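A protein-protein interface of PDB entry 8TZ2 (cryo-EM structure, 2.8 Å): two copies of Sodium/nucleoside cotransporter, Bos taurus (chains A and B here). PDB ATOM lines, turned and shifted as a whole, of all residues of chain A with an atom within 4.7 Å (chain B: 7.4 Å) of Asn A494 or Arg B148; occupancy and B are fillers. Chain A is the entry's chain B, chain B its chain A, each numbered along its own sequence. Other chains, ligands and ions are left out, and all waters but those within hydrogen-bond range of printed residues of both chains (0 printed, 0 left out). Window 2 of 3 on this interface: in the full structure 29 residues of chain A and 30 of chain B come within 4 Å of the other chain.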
ATOM      1  N   SER A 490      25.486  -1.082  35.483  1.00  0.00           N
ATOM      2  CA  SER A 490      25.420  -2.516  35.224  1.00  0.00           C
ATOM      3  C   SER A 490      25.302  -2.793  33.732  1.00  0.00           C
ATOM      4  O   SER A 490      25.888  -3.754  33.221  1.00  0.00           O
ATOM      5  CB  SER A 490      24.251  -3.136  35.979  1.00  0.00           C
ATOM      6  OG  SER A 490      24.297  -4.548  35.912  1.00  0.00           O
ATOM      7  N   TRP A 491      24.542  -1.961  33.016  1.00  0.00           N
ATOM      8  CA  TRP A 491      24.439  -2.107  31.569  1.00  0.00           C
ATOM      9  C   TRP A 491      25.796  -1.928  30.898  1.00  0.00           C
ATOM     10  O   TRP A 491      26.154  -2.684  29.989  1.00  0.00           O
ATOM     11  CB  TRP A 491      23.425  -1.099  31.032  1.00  0.00           C
ATOM     12  CG  TRP A 491      23.337  -1.023  29.549  1.00  0.00           C
ATOM     13  CD1 TRP A 491      22.675  -1.879  28.723  1.00  0.00           C
ATOM     14  CD2 TRP A 491      23.914  -0.018  28.709  1.00  0.00           C
ATOM     15  NE1 TRP A 491      22.811  -1.475  27.419  1.00  0.00           N
ATOM     16  CE2 TRP A 491      23.567  -0.334  27.384  1.00  0.00           C
ATOM     17  CE3 TRP A 491      24.693   1.115  28.951  1.00  0.00           C
ATOM     18  CZ2 TRP A 491      23.973   0.440  26.304  1.00  0.00           C
ATOM     19  CZ3 TRP A 491      25.094   1.882  27.879  1.00  0.00           C
ATOM     20  CH2 TRP A 491      24.734   1.543  26.572  1.00  0.00           C
ATOM     21  N   LEU A 492      26.566  -0.930  31.337  1.00  0.00           N
ATOM     22  CA  LEU A 492      27.900  -0.721  30.783  1.00  0.00           C
ATOM     23  C   LEU A 492      28.863  -1.815  31.226  1.00  0.00           C
ATOM     24  O   LEU A 492      29.662  -2.309  30.423  1.00  0.00           O
ATOM     25  CB  LEU A 492      28.426   0.652  31.201  1.00  0.00           C
ATOM     26  CG  LEU A 492      29.916   0.923  30.986  1.00  0.00           C
ATOM     27  CD1 LEU A 492      30.291   0.817  29.524  1.00  0.00           C
ATOM     28  CD2 LEU A 492      30.275   2.287  31.533  1.00  0.00           C
ATOM     29  N   GLY A 493      28.806  -2.202  32.500  1.00  0.00           N
ATOM     30  CA  GLY A 493      29.740  -3.193  33.004  1.00  0.00           C
ATOM     31  C   GLY A 493      29.585  -4.550  32.352  1.00  0.00           C
ATOM     32  O   GLY A 493      30.571  -5.268  32.169  1.00  0.00           O
ATOM     33  N   ASN A 494      28.356  -4.924  31.997  1.00  0.00           N
ATOM     34  CA  ASN A 494      28.131  -6.227  31.384  1.00  0.00           C
ATOM     35  C   ASN A 494      28.873  -6.374  30.064  1.00  0.00           C
ATOM     36  O   ASN A 494      29.095  -7.503  29.612  1.00  0.00           O
ATOM     37  CB  ASN A 494      26.639  -6.457  31.157  1.00  0.00           C
ATOM     38  CG  ASN A 494      26.332  -7.861  30.689  1.00  0.00           C
ATOM     39  OD1 ASN A 494      26.991  -8.819  31.089  1.00  0.00           O
ATOM     40  ND2 ASN A 494      25.331  -7.990  29.831  1.00  0.00           N
ATOM     41  N   MET A 495      29.261  -5.265  29.438  1.00  0.00           N
ATOM     42  CA  MET A 495      30.039  -5.325  28.211  1.00  0.00           C
ATOM     43  C   MET A 495      31.470  -5.780  28.454  1.00  0.00           C
ATOM     44  O   MET A 495      32.177  -6.090  27.488  1.00  0.00           O
ATOM     45  CB  MET A 495      30.031  -3.959  27.528  1.00  0.00           C
ATOM     46  CG  MET A 495      28.647  -3.487  27.125  1.00  0.00           C
ATOM     47  SD  MET A 495      28.645  -1.899  26.281  1.00  0.00           S
ATOM     48  CE  MET A 495      26.891  -1.690  25.998  1.00  0.00           C
ATOM     49  N   PHE A 496      31.911  -5.826  29.713  1.00  0.00           N
ATOM     50  CA  PHE A 496      33.223  -6.347  30.082  1.00  0.00           C
ATOM     51  C   PHE A 496      33.108  -7.541  31.019  1.00  0.00           C
ATOM     52  O   PHE A 496      34.055  -7.845  31.750  1.00  0.00           O
ATOM     53  CB  PHE A 496      34.073  -5.255  30.731  1.00  0.00           C
ATOM     54  CG  PHE A 496      34.046  -3.948  30.000  1.00  0.00           C
ATOM     55  CD1 PHE A 496      33.122  -2.976  30.336  1.00  0.00           C
ATOM     56  CD2 PHE A 496      34.943  -3.689  28.981  1.00  0.00           C
ATOM     57  CE1 PHE A 496      33.093  -1.772  29.668  1.00  0.00           C
ATOM     58  CE2 PHE A 496      34.917  -2.486  28.310  1.00  0.00           C
ATOM     59  CZ  PHE A 496      33.992  -1.526  28.653  1.00  0.00           C
ATOM     60  N   ASP A 497      31.961  -8.218  31.018  1.00  0.00           N
ATOM     61  CA  ASP A 497      31.719  -9.361  31.897  1.00  0.00           C
ATOM     62  C   ASP A 497      31.795  -8.967  33.369  1.00  0.00           C
ATOM     63  O   ASP A 497      32.176  -9.777  34.219  1.00  0.00           O
ATOM     64  CB  ASP A 497      32.700 -10.497  31.601  1.00  0.00           C
ATOM     65  CG  ASP A 497      32.589 -11.008  30.181  1.00  0.00           C
ATOM     66  OD1 ASP A 497      31.450 -11.217  29.713  1.00  0.00           O
ATOM     67  OD2 ASP A 497      33.642 -11.192  29.531  1.00  0.00           O
ATOM     68  N   TYR A 498      31.439  -7.724  33.686  1.00  0.00           N
ATOM     69  CA  TYR A 498      31.403  -7.230  35.063  1.00  0.00           C
ATOM     70  C   TYR A 498      30.089  -6.497  35.294  1.00  0.00           C
ATOM     71  O   TYR A 498      30.060  -5.269  35.436  1.00  0.00           O
ATOM     72  CB  TYR A 498      32.599  -6.324  35.353  1.00  0.00           C
ATOM     73  CG  TYR A 498      32.793  -6.023  36.821  1.00  0.00           C
ATOM     74  CD1 TYR A 498      32.993  -7.044  37.736  1.00  0.00           C
ATOM     75  CD2 TYR A 498      32.789  -4.718  37.290  1.00  0.00           C
ATOM     76  CE1 TYR A 498      33.172  -6.776  39.074  1.00  0.00           C
ATOM     77  CE2 TYR A 498      32.968  -4.443  38.628  1.00  0.00           C
ATOM     78  CZ  TYR A 498      33.158  -5.476  39.516  1.00  0.00           C
ATOM     79  OH  TYR A 498      33.339  -5.207  40.853  1.00  0.00           O
ATOM     80  N   PRO A 499      28.970  -7.227  35.335  1.00  0.00           N
ATOM     81  CA  PRO A 499      27.675  -6.588  35.605  1.00  0.00           C
ATOM     82  C   PRO A 499      27.479  -6.163  37.051  1.00  0.00           C
ATOM     83  O   PRO A 499      26.406  -5.648  37.383  1.00  0.00           O
ATOM     84  CB  PRO A 499      26.666  -7.673  35.207  1.00  0.00           C
ATOM     85  CG  PRO A 499      27.394  -8.944  35.382  1.00  0.00           C
ATOM     86  CD  PRO A 499      28.826  -8.661  35.038  1.00  0.00           C
ATOM     87  N   ALA B 140      37.419  -1.329  23.571  1.00  0.00           N
ATOM     88  CA  ALA B 140      37.614  -2.592  24.270  1.00  0.00           C
ATOM     89  C   ALA B 140      36.308  -3.371  24.375  1.00  0.00           C
ATOM     90  O   ALA B 140      36.289  -4.594  24.192  1.00  0.00           O
ATOM     91  CB  ALA B 140      38.198  -2.336  25.656  1.00  0.00           C
ATOM     92  N   ALA B 141      35.204  -2.680  24.668  1.00  0.00           N
ATOM     93  CA  ALA B 141      33.915  -3.356  24.753  1.00  0.00           C
ATOM     94  C   ALA B 141      33.548  -3.988  23.418  1.00  0.00           C
ATOM     95  O   ALA B 141      33.052  -5.119  23.366  1.00  0.00           O
ATOM     96  CB  ALA B 141      32.837  -2.369  25.200  1.00  0.00           C
ATOM     97  N   CYS B 142      33.783  -3.264  22.323  1.00  0.00           N
ATOM     98  CA  CYS B 142      33.504  -3.824  21.003  1.00  0.00           C
ATOM     99  C   CYS B 142      34.400  -5.022  20.711  1.00  0.00           C
ATOM    100  O   CYS B 142      33.954  -6.012  20.120  1.00  0.00           O
ATOM    101  CB  CYS B 142      33.678  -2.751  19.930  1.00  0.00           C
ATOM    102  SG  CYS B 142      32.468  -1.412  20.009  1.00  0.00           S
ATOM    103  N   MET B 144      35.831  -7.165  22.878  1.00  0.00           N
ATOM    104  CA  MET B 144      35.419  -8.335  23.649  1.00  0.00           C
ATOM    105  C   MET B 144      34.163  -8.962  23.059  1.00  0.00           C
ATOM    106  O   MET B 144      34.065 -10.189  22.945  1.00  0.00           O
ATOM    107  CB  MET B 144      35.191  -7.952  25.111  1.00  0.00           C
ATOM    108  CG  MET B 144      36.428  -7.424  25.823  1.00  0.00           C
ATOM    109  SD  MET B 144      36.158  -7.144  27.584  1.00  0.00           S
ATOM    110  CE  MET B 144      35.861  -8.815  28.157  1.00  0.00           C
ATOM    111  N   ASN B 145      33.191  -8.135  22.679  1.00  0.00           N
ATOM    112  CA  ASN B 145      31.982  -8.610  22.022  1.00  0.00           C
ATOM    113  C   ASN B 145      31.287  -7.439  21.341  1.00  0.00           C
ATOM    114  O   ASN B 145      31.032  -6.409  21.974  1.00  0.00           O
ATOM    115  CB  ASN B 145      31.049  -9.290  23.025  1.00  0.00           C
ATOM    116  CG  ASN B 145      29.833  -9.913  22.367  1.00  0.00           C
ATOM    117  OD1 ASN B 145      29.425  -9.513  21.276  1.00  0.00           O
ATOM    118  ND2 ASN B 145      29.244 -10.898  23.032  1.00  0.00           N
ATOM    119  N   PHE B 146      30.978  -7.584  20.055  1.00  0.00           N
ATOM    120  CA  PHE B 146      30.445  -6.480  19.267  1.00  0.00           C
ATOM    121  C   PHE B 146      28.924  -6.395  19.347  1.00  0.00           C
ATOM    122  O   PHE B 146      28.370  -5.308  19.534  1.00  0.00           O
ATOM    123  CB  PHE B 146      30.886  -6.620  17.810  1.00  0.00           C
ATOM    124  CG  PHE B 146      30.682  -5.379  17.000  1.00  0.00           C
ATOM    125  CD1 PHE B 146      31.690  -4.438  16.889  1.00  0.00           C
ATOM    126  CD2 PHE B 146      29.480  -5.147  16.354  1.00  0.00           C
ATOM    127  CE1 PHE B 146      31.504  -3.291  16.145  1.00  0.00           C
ATOM    128  CE2 PHE B 146      29.290  -4.002  15.609  1.00  0.00           C
ATOM    129  CZ  PHE B 146      30.304  -3.073  15.505  1.00  0.00           C
ATOM    130  N   HIS B 147      28.236  -7.529  19.204  1.00  0.00           N
ATOM    131  CA  HIS B 147      26.777  -7.511  19.239  1.00  0.00           C
ATOM    132  C   HIS B 147      26.267  -7.001  20.579  1.00  0.00           C
ATOM    133  O   HIS B 147      25.230  -6.331  20.643  1.00  0.00           O
ATOM    134  CB  HIS B 147      26.233  -8.910  18.954  1.00  0.00           C
ATOM    135  CG  HIS B 147      24.739  -8.995  18.979  1.00  0.00           C
ATOM    136  ND1 HIS B 147      23.939  -8.316  18.087  1.00  0.00           N
ATOM    137  CD2 HIS B 147      23.899  -9.684  19.789  1.00  0.00           C
ATOM    138  CE1 HIS B 147      22.671  -8.581  18.346  1.00  0.00           C
ATOM    139  NE2 HIS B 147      22.620  -9.408  19.374  1.00  0.00           N
ATOM    140  N   ARG B 148      26.983  -7.311  21.661  1.00  0.00           N
ATOM    141  CA  ARG B 148      26.577  -6.855  22.984  1.00  0.00           C
ATOM    142  C   ARG B 148      26.859  -5.371  23.183  1.00  0.00           C
ATOM    143  O   ARG B 148      26.148  -4.705  23.943  1.00  0.00           O
ATOM    144  CB  ARG B 148      27.296  -7.684  24.049  1.00  0.00           C
ATOM    145  CG  ARG B 148      26.836  -7.443  25.470  1.00  0.00           C
ATOM    146  CD  ARG B 148      27.501  -8.425  26.417  1.00  0.00           C
ATOM    147  NE  ARG B 148      28.954  -8.402  26.295  1.00  0.00           N
ATOM    148  CZ  ARG B 148      29.770  -9.259  26.892  1.00  0.00           C
ATOM    149  NH1 ARG B 148      29.311 -10.233  27.660  1.00  0.00           N
ATOM    150  NH2 ARG B 148      31.082  -9.136  26.714  1.00  0.00           N
ATOM    151  N   ALA B 149      27.880  -4.839  22.514  1.00  0.00           N
ATOM    152  CA  ALA B 149      28.303  -3.454  22.675  1.00  0.00           C
ATOM    153  C   ALA B 149      27.789  -2.542  21.568  1.00  0.00           C
ATOM    154  O   ALA B 149      28.236  -1.396  21.467  1.00  0.00           O
ATOM    155  CB  ALA B 149      29.828  -3.376  22.733  1.00  0.00           C
ATOM    156  N   LEU B 150      26.869  -3.023  20.736  1.00  0.00           N
ATOM    157  CA  LEU B 150      26.424  -2.239  19.584  1.00  0.00           C
ATOM    158  C   LEU B 150      25.798  -0.907  19.973  1.00  0.00           C
ATOM    159  O   LEU B 150      26.185   0.124  19.392  1.00  0.00           O
ATOM    160  CB  LEU B 150      25.453  -3.080  18.752  1.00  0.00           C
ATOM    161  CG  LEU B 150      25.056  -2.510  17.390  1.00  0.00           C
ATOM    162  CD1 LEU B 150      26.245  -2.516  16.450  1.00  0.00           C
ATOM    163  CD2 LEU B 150      23.899  -3.298  16.796  1.00  0.00           C
ATOM    164  N   PRO B 151      24.836  -0.842  20.899  1.00  0.00           N
ATOM    165  CA  PRO B 151      24.207   0.459  21.196  1.00  0.00           C
ATOM    166  C   PRO B 151      25.187   1.519  21.663  1.00  0.00           C
ATOM    167  O   PRO B 151      25.046   2.694  21.298  1.00  0.00           O
ATOM    168  CB  PRO B 151      23.182   0.112  22.287  1.00  0.00           C
ATOM    169  CG  PRO B 151      23.557  -1.239  22.786  1.00  0.00           C
ATOM    170  CD  PRO B 151      24.214  -1.940  21.654  1.00  0.00           C
ATOM    171  N   LEU B 152      26.184   1.137  22.458  1.00  0.00           N
ATOM    172  CA  LEU B 152      27.182   2.103  22.899  1.00  0.00           C
ATOM    173  C   LEU B 152      27.951   2.662  21.708  1.00  0.00           C
ATOM    174  O   LEU B 152      28.199   3.872  21.625  1.00  0.00           O
ATOM    175  CB  LEU B 152      28.129   1.437  23.894  1.00  0.00           C
ATOM    176  CG  LEU B 152      29.235   2.283  24.517  1.00  0.00           C
ATOM    177  CD1 LEU B 152      28.665   3.403  25.361  1.00  0.00           C
ATOM    178  CD2 LEU B 152      30.115   1.382  25.351  1.00  0.00           C
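The guanidinium group (NH1) of Arg B148 sits close to the backbone carbonyl oxygen (O) of Asn A494 (3.4 Å).
NH2 of Arg B148 lies within hydrogen-bond range of O of Met A495.
OD1 of Asp A497 lies within salt-bridge range of NH1 of Arg B148, 3.1 Å away.
The side-chain amide oxygen of Asn B145 lies within hydrogen-bond range of the backbone NH of Arg B148 (3.3 Å).
CZ2 of Trp A491 touches CG of Pro B151 (3.9 Å).
Met A495 touches Ala B141 (CB to CB, 3.98 Å).
Met A495 touches Ala B149.
Met A495 touches Leu B152 (SD to CD2, 3.7 Å).
N of Ala B141 touches CE2 of Phe A496, at 3.7 Å.
CD2 of Phe A496 touches SD of Met B144, at 3.9 Å.
Asp A497 touches Met B144 (OD2 to CE, 3.5 Å).
Asn A494 touches one residue of chain B.
Printed residues of chain A within 4 Å of Arg B148: Asn A494 (3.3 Å), Met A495 (3.3 Å) and Asp A497 (3.1 Å).
Of the printed residues of chain A, Pro B151 touches Trp A491.
Of the printed residues of chain A, Leu B152 touches Met A495 (3.7 Å).
Printed residues of chain B within 4 Å of Phe A496: Ala B141 and Met B144.
Of the printed residues of chain A, Ala B149 touches Met A495 (3.9 Å).
The nearest residue of chain B that does not touch Asn A494 is Met B144 (7.0 Å).
The nearest residue of chain A that does not touch Arg B148 is Phe A496 (4.5 Å).
Hydrophobic or aromatic side chains of chain B within 4 Å of the printed part of chain A: Ala B141, Met B144, Pro B151 and Leu B152.
Among the printed residues, 10 pairs touch across the chains.
No position is printed for both chains.
Of the 10 pairs that touch across the chains among the printed residues, none has its exchanged pair printed and touching as well.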
